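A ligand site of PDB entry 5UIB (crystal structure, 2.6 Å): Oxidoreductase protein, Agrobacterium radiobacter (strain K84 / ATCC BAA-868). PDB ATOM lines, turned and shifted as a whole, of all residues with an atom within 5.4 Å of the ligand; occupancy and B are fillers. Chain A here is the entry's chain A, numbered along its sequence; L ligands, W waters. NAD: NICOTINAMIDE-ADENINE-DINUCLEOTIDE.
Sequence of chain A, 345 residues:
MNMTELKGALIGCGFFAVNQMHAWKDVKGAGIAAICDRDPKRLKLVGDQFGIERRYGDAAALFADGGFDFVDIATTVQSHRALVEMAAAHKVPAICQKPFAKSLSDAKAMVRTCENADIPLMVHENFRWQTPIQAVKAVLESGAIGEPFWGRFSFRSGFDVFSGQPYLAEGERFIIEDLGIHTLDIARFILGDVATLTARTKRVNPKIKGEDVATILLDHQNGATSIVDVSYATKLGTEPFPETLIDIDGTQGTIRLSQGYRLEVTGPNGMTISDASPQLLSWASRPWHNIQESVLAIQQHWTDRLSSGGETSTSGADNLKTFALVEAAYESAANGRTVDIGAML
OD1 of Asp 178 is in salt-bridge range of NZ of Lys 98 (3.4 Å).
OD1 of Asp 37 sits at hydrogen-bond distance from N of Asp 39, 2.7 Å away.
A ring nitrogen (NE2) of His 124 is in hydrogen-bond range of the side-chain amide nitrogen of Asn 126, 3.0 Å away.
The side-chain hydroxyl (OH) of Tyr 167 sits at hydrogen-bond distance from the side-chain amide nitrogen (NE2) of Gln 165 (2.6 Å).
The backbone carbonyl oxygen (O) of Thr 75 lies within hydrogen-bond range of a ring nitrogen (NE2) of His 80 (2.6 Å).
The backbone NH of Gly 12 sits at hydrogen-bond distance from the backbone carbonyl oxygen of Cys 36 (3.0 Å).
The backbone NH (N) of Ala 74 lies within hydrogen-bond range of the backbone carbonyl oxygen (O) of Ile 11, at 2.8 Å.
The guanidinium group (NE) of Arg 42 is in hydrogen-bond range of the backbone carbonyl oxygen (O) of Cys 13.
The backbone carbonyl oxygen (O) of Lys 98 lies within hydrogen-bond range of an oxygen (O2D) of the ligand (2.6 Å).
NZ of Lys 98 sits at hydrogen-bond distance from O2D of the ligand.
OD1 of Asp 37 is in hydrogen-bond range of O2B of the ligand, at 2.8 Å.
ND2 of Asn 126 lies within hydrogen-bond range of O7N of the ligand.
OG of Ser 79 is in hydrogen-bond range of N7A of the ligand, 2.8 Å away.
The side-chain hydroxyl of Tyr 167 sits at hydrogen-bond distance from an oxygen (O1N) of the ligand.
N of Phe 15 is in hydrogen-bond range of O2A of the ligand (2.9 Å).
The backbone NH (N) of Phe 16 lies within hydrogen-bond range of an oxygen (O2N) of the ligand (3.0 Å).
O7N of the ligand sits at hydrogen-bond distance from NE2 of Gln 97 (3.3 Å).
Water W1 lies within hydrogen-bond range of O of Ala 74, O2N of the ligand, N of Gly 14 and O of Gly 12.
Merely in contact with the ligand: Gly 14 (3.3 Å), Thr 75 (3.4 Å), Gly 12 (3.4 Å), Pro 99 (3.5 Å), Ala 74 (3.5 Å), Arg 38 (3.6 Å), Gln 165 (3.6 Å), Thr 76 (3.6 Å), His 182 (3.7 Å), Asp 39 (3.7 Å), Ile 11 (3.7 Å), His 124 (3.9 Å), Ile 291 (3.9 Å) and Arg 42 (3.96 Å).
Hydrophobic or aromatic side chains that line the ligand: Ile 11, Phe 15, Phe 16, Pro 99, His 124, Tyr 167, His 182 and Ile 291.
The nearest printed residue that does not touch the ligand is Cys 36 (4.03 Å).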
ATOM      1  N   ILE A  11       3.369  -8.952  21.789  1.00  0.00           N
ATOM      2  CA  ILE A  11       2.454 -10.076  21.772  1.00  0.00           C
ATOM      3  C   ILE A  11       1.948 -10.236  20.344  1.00  0.00           C
ATOM      4  O   ILE A  11       1.297  -9.357  19.813  1.00  0.00           O
ATOM      5  CB  ILE A  11       1.273  -9.861  22.734  1.00  0.00           C
ATOM      6  CG1 ILE A  11       1.779  -9.730  24.180  1.00  0.00           C
ATOM      7  CG2 ILE A  11       0.270 -11.003  22.610  1.00  0.00           C
ATOM      8  CD1 ILE A  11       0.783  -9.105  25.133  1.00  0.00           C
ATOM      9  N   GLY A  12       2.273 -11.380  19.741  1.00  0.00           N
ATOM     10  CA  GLY A  12       1.851 -11.726  18.386  1.00  0.00           C
ATOM     11  C   GLY A  12       3.004 -11.616  17.417  1.00  0.00           C
ATOM     12  O   GLY A  12       3.092 -10.655  16.677  1.00  0.00           O
ATOM     13  N   CYS A  13       3.865 -12.631  17.422  1.00  0.00           N
ATOM     14  CA  CYS A  13       5.093 -12.653  16.612  1.00  0.00           C
ATOM     15  C   CYS A  13       4.843 -13.123  15.181  1.00  0.00           C
ATOM     16  O   CYS A  13       5.496 -14.060  14.714  1.00  0.00           O
ATOM     17  CB  CYS A  13       6.116 -13.576  17.275  1.00  0.00           C
ATOM     18  SG  CYS A  13       6.567 -13.064  18.935  1.00  0.00           S
ATOM     19  N   GLY A  14       3.924 -12.462  14.497  1.00  0.00           N
ATOM     20  CA  GLY A  14       3.419 -12.936  13.222  1.00  0.00           C
ATOM     21  C   GLY A  14       4.207 -12.421  12.040  1.00  0.00           C
ATOM     22  O   GLY A  14       5.393 -12.135  12.158  1.00  0.00           O
ATOM     23  N   PHE A  15       3.511 -12.304  10.915  1.00  0.00           N
ATOM     24  CA  PHE A  15       4.109 -11.932   9.624  1.00  0.00           C
ATOM     25  C   PHE A  15       4.576 -10.472   9.654  1.00  0.00           C
ATOM     26  O   PHE A  15       5.739 -10.182   9.369  1.00  0.00           O
ATOM     27  CB  PHE A  15       3.120 -12.267   8.455  1.00  0.00           C
ATOM     28  CG  PHE A  15       3.267 -11.399   7.203  1.00  0.00           C
ATOM     29  CD1 PHE A  15       4.264 -11.661   6.245  1.00  0.00           C
ATOM     30  CD2 PHE A  15       2.382 -10.327   6.966  1.00  0.00           C
ATOM     31  CE1 PHE A  15       4.384 -10.861   5.105  1.00  0.00           C
ATOM     32  CE2 PHE A  15       2.492  -9.541   5.821  1.00  0.00           C
ATOM     33  CZ  PHE A  15       3.498  -9.796   4.891  1.00  0.00           C
ATOM     34  N   PHE A  16       3.669  -9.579  10.049  1.00  0.00           N
ATOM     35  CA  PHE A  16       3.950  -8.139  10.121  1.00  0.00           C
ATOM     36  C   PHE A  16       4.741  -7.727  11.365  1.00  0.00           C
ATOM     37  O   PHE A  16       5.425  -6.707  11.350  1.00  0.00           O
ATOM     38  CB  PHE A  16       2.655  -7.329  10.045  1.00  0.00           C
ATOM     39  CG  PHE A  16       2.874  -5.863   9.763  1.00  0.00           C
ATOM     40  CD1 PHE A  16       3.226  -5.434   8.491  1.00  0.00           C
ATOM     41  CD2 PHE A  16       2.747  -4.905  10.771  1.00  0.00           C
ATOM     42  CE1 PHE A  16       3.420  -4.086   8.214  1.00  0.00           C
ATOM     43  CE2 PHE A  16       2.954  -3.554  10.500  1.00  0.00           C
ATOM     44  CZ  PHE A  16       3.285  -3.151   9.220  1.00  0.00           C
ATOM     45  N   ALA A  17       4.658  -8.511  12.436  1.00  0.00           N
ATOM     46  CA  ALA A  17       5.392  -8.186  13.666  1.00  0.00           C
ATOM     47  C   ALA A  17       6.899  -8.152  13.466  1.00  0.00           C
ATOM     48  O   ALA A  17       7.605  -7.455  14.213  1.00  0.00           O
ATOM     49  CB  ALA A  17       5.035  -9.179  14.756  1.00  0.00           C
ATOM     50  N   CYS A  36       5.807 -12.775  23.041  1.00  0.00           N
ATOM     51  CA  CYS A  36       4.744 -13.714  23.349  1.00  0.00           C
ATOM     52  C   CYS A  36       4.141 -14.261  22.068  1.00  0.00           C
ATOM     53  O   CYS A  36       3.958 -13.510  21.110  1.00  0.00           O
ATOM     54  CB  CYS A  36       3.675 -12.996  24.161  1.00  0.00           C
ATOM     55  SG  CYS A  36       2.327 -14.076  24.700  1.00  0.00           S
ATOM     56  N   ASP A  37       3.857 -15.557  22.048  1.00  0.00           N
ATOM     57  CA  ASP A  37       3.085 -16.164  20.965  1.00  0.00           C
ATOM     58  C   ASP A  37       2.583 -17.560  21.318  1.00  0.00           C
ATOM     59  O   ASP A  37       3.335 -18.364  21.864  1.00  0.00           O
ATOM     60  CB  ASP A  37       3.917 -16.242  19.669  1.00  0.00           C
ATOM     61  CG  ASP A  37       3.048 -16.172  18.427  1.00  0.00           C
ATOM     62  OD1 ASP A  37       2.317 -17.158  18.168  1.00  0.00           O
ATOM     63  OD2 ASP A  37       3.078 -15.130  17.739  1.00  0.00           O
ATOM     64  N   ARG A  38       1.325 -17.831  20.971  1.00  0.00           N
ATOM     65  CA  ARG A  38       0.749 -19.186  21.067  1.00  0.00           C
ATOM     66  C   ARG A  38       1.363 -20.200  20.115  1.00  0.00           C
ATOM     67  O   ARG A  38       1.183 -21.405  20.309  1.00  0.00           O
ATOM     68  CB  ARG A  38      -0.738 -19.164  20.762  1.00  0.00           C
ATOM     69  CG  ARG A  38      -1.570 -18.477  21.811  1.00  0.00           C
ATOM     70  CD  ARG A  38      -2.935 -18.202  21.222  1.00  0.00           C
ATOM     71  NE  ARG A  38      -3.948 -17.984  22.238  1.00  0.00           N
ATOM     72  CZ  ARG A  38      -5.223 -17.715  21.967  1.00  0.00           C
ATOM     73  NH1 ARG A  38      -5.646 -17.620  20.697  1.00  0.00           N
ATOM     74  NH2 ARG A  38      -6.088 -17.544  22.959  1.00  0.00           N
ATOM     75  N   ASP A  39       2.019 -19.731  19.061  1.00  0.00           N
ATOM     76  CA  ASP A  39       2.616 -20.618  18.083  1.00  0.00           C
ATOM     77  C   ASP A  39       4.119 -20.702  18.377  1.00  0.00           C
ATOM     78  O   ASP A  39       4.871 -19.828  17.946  1.00  0.00           O
ATOM     79  CB  ASP A  39       2.350 -20.048  16.689  1.00  0.00           C
ATOM     80  CG  ASP A  39       2.751 -20.999  15.583  1.00  0.00           C
ATOM     81  OD1 ASP A  39       3.286 -22.107  15.842  1.00  0.00           O
ATOM     82  OD2 ASP A  39       2.513 -20.598  14.417  1.00  0.00           O
ATOM     83  N   ARG A  42       6.680 -19.643  15.698  1.00  0.00           N
ATOM     84  CA  ARG A  42       6.856 -18.201  15.500  1.00  0.00           C
ATOM     85  C   ARG A  42       7.578 -17.546  16.673  1.00  0.00           C
ATOM     86  O   ARG A  42       8.407 -16.656  16.473  1.00  0.00           O
ATOM     87  CB  ARG A  42       5.498 -17.530  15.306  1.00  0.00           C
ATOM     88  CG  ARG A  42       4.747 -17.968  14.045  1.00  0.00           C
ATOM     89  CD  ARG A  42       5.478 -17.597  12.766  1.00  0.00           C
ATOM     90  NE  ARG A  42       5.866 -16.179  12.767  1.00  0.00           N
ATOM     91  CZ  ARG A  42       6.680 -15.612  11.898  1.00  0.00           C
ATOM     92  NH1 ARG A  42       7.211 -16.320  10.895  1.00  0.00           N
ATOM     93  NH2 ARG A  42       6.965 -14.318  12.015  1.00  0.00           N
ATOM     94  N   ALA A  59       0.066 -14.941  26.968  1.00  0.00           N
ATOM     95  CA  ALA A  59       0.168 -13.533  27.405  1.00  0.00           C
ATOM     96  C   ALA A  59      -0.137 -13.300  28.896  1.00  0.00           C
ATOM     97  O   ALA A  59       0.337 -12.311  29.460  1.00  0.00           O
ATOM     98  CB  ALA A  59      -0.715 -12.660  26.538  1.00  0.00           C
ATOM     99  N   ALA A  74       0.427  -7.124  18.432  1.00  0.00           N
ATOM    100  CA  ALA A  74       0.439  -7.356  16.990  1.00  0.00           C
ATOM    101  C   ALA A  74      -0.314  -8.645  16.576  1.00  0.00           C
ATOM    102  O   ALA A  74      -0.055  -9.194  15.500  1.00  0.00           O
ATOM    103  CB  ALA A  74       1.878  -7.382  16.481  1.00  0.00           C
ATOM    104  N   THR A  75      -1.254  -9.100  17.403  1.00  0.00           N
ATOM    105  CA  THR A  75      -2.082 -10.265  17.068  1.00  0.00           C
ATOM    106  C   THR A  75      -3.179  -9.796  16.163  1.00  0.00           C
ATOM    107  O   THR A  75      -3.354  -8.575  16.001  1.00  0.00           O
ATOM    108  CB  THR A  75      -2.748 -10.900  18.306  1.00  0.00           C
ATOM    109  OG1 THR A  75      -3.661  -9.964  18.886  1.00  0.00           O
ATOM    110  CG2 THR A  75      -1.708 -11.321  19.313  1.00  0.00           C
ATOM    111  N   THR A  76      -3.933 -10.749  15.602  1.00  0.00           N
ATOM    112  CA  THR A  76      -5.152 -10.446  14.831  1.00  0.00           C
ATOM    113  C   THR A  76      -6.286 -10.018  15.769  1.00  0.00           C
ATOM    114  O   THR A  76      -6.200 -10.191  16.991  1.00  0.00           O
ATOM    115  CB  THR A  76      -5.604 -11.642  13.967  1.00  0.00           C
ATOM    116  OG1 THR A  76      -5.785 -12.792  14.793  1.00  0.00           O
ATOM    117  CG2 THR A  76      -4.583 -11.937  12.913  1.00  0.00           C
ATOM    118  N   VAL A  77      -7.358  -9.498  15.168  1.00  0.00           N
ATOM    119  CA  VAL A  77      -8.437  -8.800  15.881  1.00  0.00           C
ATOM    120  C   VAL A  77      -9.110  -9.564  17.045  1.00  0.00           C
ATOM    121  O   VAL A  77      -9.582  -8.946  17.998  1.00  0.00           O
ATOM    122  CB  VAL A  77      -9.528  -8.317  14.875  1.00  0.00           C
ATOM    123  CG1 VAL A  77     -10.366  -9.492  14.384  1.00  0.00           C
ATOM    124  CG2 VAL A  77     -10.390  -7.232  15.478  1.00  0.00           C
ATOM    125  N   SER A  79      -7.937 -11.471  19.521  1.00  0.00           N
ATOM    126  CA  SER A  79      -7.285 -11.267  20.806  1.00  0.00           C
ATOM    127  C   SER A  79      -7.244  -9.820  21.295  1.00  0.00           C
ATOM    128  O   SER A  79      -6.989  -9.572  22.468  1.00  0.00           O
ATOM    129  CB  SER A  79      -5.843 -11.792  20.744  1.00  0.00           C
ATOM    130  OG  SER A  79      -5.743 -12.939  19.921  1.00  0.00           O
ATOM    131  N   HIS A  80      -7.478  -8.861  20.398  1.00  0.00           N
ATOM    132  CA  HIS A  80      -7.276  -7.442  20.726  1.00  0.00           C
ATOM    133  C   HIS A  80      -7.941  -6.928  22.001  1.00  0.00           C
ATOM    134  O   HIS A  80      -7.286  -6.290  22.823  1.00  0.00           O
ATOM    135  CB  HIS A  80      -7.704  -6.565  19.543  1.00  0.00           C
ATOM    136  CG  HIS A  80      -6.736  -6.584  18.417  1.00  0.00           C
ATOM    137  ND1 HIS A  80      -6.804  -5.694  17.355  1.00  0.00           N
ATOM    138  CD2 HIS A  80      -5.648  -7.356  18.193  1.00  0.00           C
ATOM    139  CE1 HIS A  80      -5.795  -5.928  16.538  1.00  0.00           C
ATOM    140  NE2 HIS A  80      -5.079  -6.937  17.017  1.00  0.00           N
ATOM    141  N   LEU A  83      -6.425  -8.551  25.301  1.00  0.00           N
ATOM    142  CA  LEU A  83      -5.040  -8.144  25.520  1.00  0.00           C
ATOM    143  C   LEU A  83      -4.940  -6.688  25.935  1.00  0.00           C
ATOM    144  O   LEU A  83      -4.104  -6.344  26.762  1.00  0.00           O
ATOM    145  CB  LEU A  83      -4.162  -8.398  24.286  1.00  0.00           C
ATOM    146  CG  LEU A  83      -3.899  -9.868  23.955  1.00  0.00           C
ATOM    147  CD1 LEU A  83      -3.235  -9.983  22.591  1.00  0.00           C
ATOM    148  CD2 LEU A  83      -3.048 -10.545  25.020  1.00  0.00           C
ATOM    149  N   GLN A  97      -2.588  -3.346  17.070  1.00  0.00           N
ATOM    150  CA  GLN A  97      -2.732  -3.354  15.609  1.00  0.00           C
ATOM    151  C   GLN A  97      -4.151  -3.056  15.150  1.00  0.00           C
ATOM    152  O   GLN A  97      -5.079  -2.923  15.945  1.00  0.00           O
ATOM    153  CB  GLN A  97      -2.227  -4.683  14.984  1.00  0.00           C
ATOM    154  CG  GLN A  97      -0.815  -4.625  14.399  1.00  0.00           C
ATOM    155  CD  GLN A  97      -0.639  -3.555  13.314  1.00  0.00           C
ATOM    156  OE1 GLN A  97      -1.617  -3.036  12.770  1.00  0.00           O
ATOM    157  NE2 GLN A  97       0.616  -3.208  13.008  1.00  0.00           N
ATOM    158  N   LYS A  98      -4.305  -2.924  13.841  1.00  0.00           N
ATOM    159  CA  LYS A  98      -5.634  -2.811  13.227  1.00  0.00           C
ATOM    160  C   LYS A  98      -6.015  -4.152  12.570  1.00  0.00           C
ATOM    161  O   LYS A  98      -5.150  -5.000  12.348  1.00  0.00           O
ATOM    162  CB  LYS A  98      -5.738  -1.606  12.282  1.00  0.00           C
ATOM    163  CG  LYS A  98      -4.554  -1.322  11.378  1.00  0.00           C
ATOM    164  CD  LYS A  98      -4.168  -2.471  10.455  1.00  0.00           C
ATOM    165  CE  LYS A  98      -5.274  -2.834   9.491  1.00  0.00           C
ATOM    166  NZ  LYS A  98      -4.976  -4.122   8.813  1.00  0.00           N
ATOM    167  N   PRO A  99      -7.314  -4.401  12.327  1.00  0.00           N
ATOM    168  CA  PRO A  99      -8.405  -3.564  12.848  1.00  0.00           C
ATOM    169  C   PRO A  99      -8.390  -3.550  14.369  1.00  0.00           C
ATOM    170  O   PRO A  99      -7.979  -4.532  15.001  1.00  0.00           O
ATOM    171  CB  PRO A  99      -9.667  -4.253  12.315  1.00  0.00           C
ATOM    172  CG  PRO A  99      -9.236  -5.605  11.870  1.00  0.00           C
ATOM    173  CD  PRO A  99      -7.801  -5.488  11.468  1.00  0.00           C
ATOM    174  N   HIS A 124      -2.024   1.168  16.225  1.00  0.00           N
ATOM    175  CA  HIS A 124      -0.981   1.117  15.179  1.00  0.00           C
ATOM    176  C   HIS A 124      -1.621   1.305  13.814  1.00  0.00           C
ATOM    177  O   HIS A 124      -1.914   0.341  13.133  1.00  0.00           O
ATOM    178  CB  HIS A 124      -0.207  -0.218  15.236  1.00  0.00           C
ATOM    179  CG  HIS A 124       1.047  -0.226  14.415  1.00  0.00           C
ATOM    180  ND1 HIS A 124       2.272  -0.562  14.945  1.00  0.00           N
ATOM    181  CD2 HIS A 124       1.275   0.078  13.106  1.00  0.00           C
ATOM    182  CE1 HIS A 124       3.204  -0.471  14.006  1.00  0.00           C
ATOM    183  NE2 HIS A 124       2.620  -0.081  12.886  1.00  0.00           N
ATOM    184  N   ASN A 126      -0.550   3.044  10.690  1.00  0.00           N
ATOM    185  CA  ASN A 126       0.680   3.619  10.130  1.00  0.00           C
ATOM    186  C   ASN A 126       0.597   4.213   8.717  1.00  0.00           C
ATOM    187  O   ASN A 126       1.579   4.773   8.238  1.00  0.00           O
ATOM    188  CB  ASN A 126       1.818   2.576  10.184  1.00  0.00           C
ATOM    189  CG  ASN A 126       1.490   1.302   9.429  1.00  0.00           C
ATOM    190  OD1 ASN A 126       0.796   1.305   8.418  1.00  0.00           O
ATOM    191  ND2 ASN A 126       1.999   0.184   9.946  1.00  0.00           N
ATOM    192  N   PHE A 127      -0.569   4.134   8.067  1.00  0.00           N
ATOM    193  CA  PHE A 127      -0.706   4.707   6.708  1.00  0.00           C
ATOM    194  C   PHE A 127      -0.524   6.233   6.681  1.00  0.00           C
ATOM    195  O   PHE A 127       0.315   6.731   5.918  1.00  0.00           O
ATOM    196  CB  PHE A 127      -2.000   4.242   6.022  1.00  0.00           C
ATOM    197  CG  PHE A 127      -1.771   3.132   5.031  1.00  0.00           C
ATOM    198  CD1 PHE A 127      -1.320   1.892   5.456  1.00  0.00           C
ATOM    199  CD2 PHE A 127      -1.983   3.325   3.671  1.00  0.00           C
ATOM    200  CE1 PHE A 127      -1.096   0.857   4.544  1.00  0.00           C
ATOM    201  CE2 PHE A 127      -1.764   2.298   2.748  1.00  0.00           C
ATOM    202  CZ  PHE A 127      -1.319   1.059   3.186  1.00  0.00           C
ATOM    203  N   GLY A 164       0.994 -13.614   1.701  1.00  0.00           N
ATOM    204  CA  GLY A 164       1.515 -13.079   2.956  1.00  0.00           C
ATOM    205  C   GLY A 164       0.522 -13.218   4.098  1.00  0.00           C
ATOM    206  O   GLY A 164       0.933 -13.507   5.226  1.00  0.00           O
ATOM    207  N   GLN A 165      -0.764 -13.041   3.789  1.00  0.00           N
ATOM    208  CA  GLN A 165      -1.849 -12.978   4.780  1.00  0.00           C
ATOM    209  C   GLN A 165      -3.051 -13.865   4.342  1.00  0.00           C
ATOM    210  O   GLN A 165      -4.060 -13.329   3.868  1.00  0.00           O
ATOM    211  CB  GLN A 165      -2.277 -11.504   4.978  1.00  0.00           C
ATOM    212  CG  GLN A 165      -1.154 -10.532   5.344  1.00  0.00           C
ATOM    213  CD  GLN A 165      -1.615  -9.083   5.559  1.00  0.00           C
ATOM    214  OE1 GLN A 165      -1.013  -8.144   5.030  1.00  0.00           O
ATOM    215  NE2 GLN A 165      -2.672  -8.885   6.347  1.00  0.00           N
ATOM    216  N   TYR A 167      -5.492 -15.417   5.846  1.00  0.00           N
ATOM    217  CA  TYR A 167      -6.794 -15.057   6.487  1.00  0.00           C
ATOM    218  C   TYR A 167      -7.650 -14.029   5.702  1.00  0.00           C
ATOM    219  O   TYR A 167      -8.883 -14.017   5.848  1.00  0.00           O
ATOM    220  CB  TYR A 167      -6.597 -14.593   7.947  1.00  0.00           C
ATOM    221  CG  TYR A 167      -5.715 -13.373   8.122  1.00  0.00           C
ATOM    222  CD1 TYR A 167      -6.227 -12.085   7.973  1.00  0.00           C
ATOM    223  CD2 TYR A 167      -4.360 -13.527   8.425  1.00  0.00           C
ATOM    224  CE1 TYR A 167      -5.405 -10.966   8.116  1.00  0.00           C
ATOM    225  CE2 TYR A 167      -3.534 -12.428   8.573  1.00  0.00           C
ATOM    226  CZ  TYR A 167      -4.056 -11.153   8.419  1.00  0.00           C
ATOM    227  OH  TYR A 167      -3.217 -10.060   8.574  1.00  0.00           O
ATOM    228  N   ASP A 178      -9.808  -4.461   6.328  1.00  0.00           N
ATOM    229  CA  ASP A 178      -8.378  -4.676   6.268  1.00  0.00           C
ATOM    230  C   ASP A 178      -7.618  -3.447   5.789  1.00  0.00           C
ATOM    231  O   ASP A 178      -6.696  -2.992   6.443  1.00  0.00           O
ATOM    232  CB  ASP A 178      -8.059  -5.830   5.335  1.00  0.00           C
ATOM    233  CG  ASP A 178      -6.578  -6.066   5.167  1.00  0.00           C
ATOM    234  OD1 ASP A 178      -5.892  -6.158   6.213  1.00  0.00           O
ATOM    235  OD2 ASP A 178      -6.100  -6.158   4.017  1.00  0.00           O
ATOM    236  N   HIS A 182      -7.421   2.063   6.535  1.00  0.00           N
ATOM    237  CA  HIS A 182      -6.323   3.008   6.388  1.00  0.00           C
ATOM    238  C   HIS A 182      -6.760   4.207   5.559  1.00  0.00           C
ATOM    239  O   HIS A 182      -6.618   5.344   5.997  1.00  0.00           O
ATOM    240  CB  HIS A 182      -5.126   2.375   5.675  1.00  0.00           C
ATOM    241  CG  HIS A 182      -4.462   1.259   6.423  1.00  0.00           C
ATOM    242  ND1 HIS A 182      -3.620   1.484   7.493  1.00  0.00           N
ATOM    243  CD2 HIS A 182      -4.479  -0.076   6.232  1.00  0.00           C
ATOM    244  CE1 HIS A 182      -3.164   0.331   7.938  1.00  0.00           C
ATOM    245  NE2 HIS A 182      -3.673  -0.638   7.186  1.00  0.00           N
ATOM    246  N   ILE A 291       5.552   1.297   3.692  1.00  0.00           N
ATOM    247  CA  ILE A 291       4.850   0.969   4.951  1.00  0.00           C
ATOM    248  C   ILE A 291       5.846   0.696   6.075  1.00  0.00           C
ATOM    249  O   ILE A 291       5.628   1.082   7.232  1.00  0.00           O
ATOM    250  CB  ILE A 291       3.940  -0.288   4.772  1.00  0.00           C
ATOM    251  CG1 ILE A 291       2.821   0.001   3.758  1.00  0.00           C
ATOM    252  CG2 ILE A 291       3.363  -0.760   6.114  1.00  0.00           C
ATOM    253  CD1 ILE A 291       2.216  -1.237   3.114  1.00  0.00           C
HETATM  254  PA  NAD L   1      -0.351 -13.335  11.647  1.00  0.00           P
HETATM  255  O1A NAD L   1      -1.364 -14.441  11.786  1.00  0.00           O
HETATM  256  O2A NAD L   1       0.881 -13.538  10.806  1.00  0.00           O
HETATM  257  O5B NAD L   1       0.123 -12.904  13.125  1.00  0.00           O
HETATM  258  C5B NAD L   1      -0.660 -13.087  14.298  1.00  0.00           C
HETATM  259  C4B NAD L   1       0.172 -13.873  15.299  1.00  0.00           C
HETATM  260  O4B NAD L   1      -0.364 -13.659  16.608  1.00  0.00           O
HETATM  261  C3B NAD L   1       0.169 -15.372  15.048  1.00  0.00           C
HETATM  262  O3B NAD L   1       1.515 -15.862  14.942  1.00  0.00           O
HETATM  263  C2B NAD L   1      -0.571 -15.979  16.237  1.00  0.00           C
HETATM  264  O2B NAD L   1       0.017 -17.212  16.661  1.00  0.00           O
HETATM  265  C1B NAD L   1      -0.446 -14.905  17.310  1.00  0.00           C
HETATM  266  N9A NAD L   1      -1.551 -14.807  18.288  1.00  0.00           N
HETATM  267  C8A NAD L   1      -2.872 -14.772  18.035  1.00  0.00           C
HETATM  268  N7A NAD L   1      -3.578 -14.641  19.192  1.00  0.00           N
HETATM  269  C5A NAD L   1      -2.696 -14.583  20.216  1.00  0.00           C
HETATM  270  C6A NAD L   1      -2.758 -14.449  21.688  1.00  0.00           C
HETATM  271  N6A NAD L   1      -3.945 -14.355  22.337  1.00  0.00           N
HETATM  272  N1A NAD L   1      -1.573 -14.434  22.369  1.00  0.00           N
HETATM  273  C2A NAD L   1      -0.378 -14.521  21.748  1.00  0.00           C
HETATM  274  N3A NAD L   1      -0.256 -14.647  20.417  1.00  0.00           N
HETATM  275  C4A NAD L   1      -1.356 -14.680  19.606  1.00  0.00           C
HETATM  276  O3  NAD L   1      -1.115 -12.023  11.118  1.00  0.00           O
HETATM  277  PN  NAD L   1      -0.327 -10.770  10.453  1.00  0.00           P
HETATM  278  O1N NAD L   1      -0.481 -10.858   8.962  1.00  0.00           O
HETATM  279  O2N NAD L   1       1.050 -10.624  11.063  1.00  0.00           O
HETATM  280  O5D NAD L   1      -1.232  -9.529  10.934  1.00  0.00           O
HETATM  281  C5D NAD L   1      -1.549  -9.341  12.311  1.00  0.00           C
HETATM  282  C4D NAD L   1      -2.319  -8.045  12.434  1.00  0.00           C
HETATM  283  O4D NAD L   1      -1.546  -6.997  11.857  1.00  0.00           O
HETATM  284  C3D NAD L   1      -3.646  -8.099  11.700  1.00  0.00           C
HETATM  285  O3D NAD L   1      -4.702  -7.660  12.556  1.00  0.00           O
HETATM  286  C2D NAD L   1      -3.495  -7.166  10.516  1.00  0.00           C
HETATM  287  O2D NAD L   1      -4.699  -6.432  10.269  1.00  0.00           O
HETATM  288  C1D NAD L   1      -2.331  -6.252  10.916  1.00  0.00           C
HETATM  289  N1N NAD L   1      -1.481  -5.751   9.816  1.00  0.00           N
HETATM  290  C2N NAD L   1      -1.189  -4.438   9.807  1.00  0.00           C
HETATM  291  C3N NAD L   1      -0.384  -3.851   8.829  1.00  0.00           C
HETATM  292  C7N NAD L   1      -0.097  -2.378   8.901  1.00  0.00           C
HETATM  293  O7N NAD L   1       0.104  -1.867   9.992  1.00  0.00           O
HETATM  294  N7N NAD L   1      -0.074  -1.634   7.794  1.00  0.00           N
HETATM  295  C4N NAD L   1       0.145  -4.673   7.834  1.00  0.00           C
HETATM  296  C5N NAD L   1      -0.161  -6.030   7.846  1.00  0.00           C
HETATM  297  C6N NAD L   1      -0.976  -6.551   8.855  1.00  0.00           C
HETATM  298  O   HOH W   1       1.875 -10.192  13.734  1.00  0.00           O
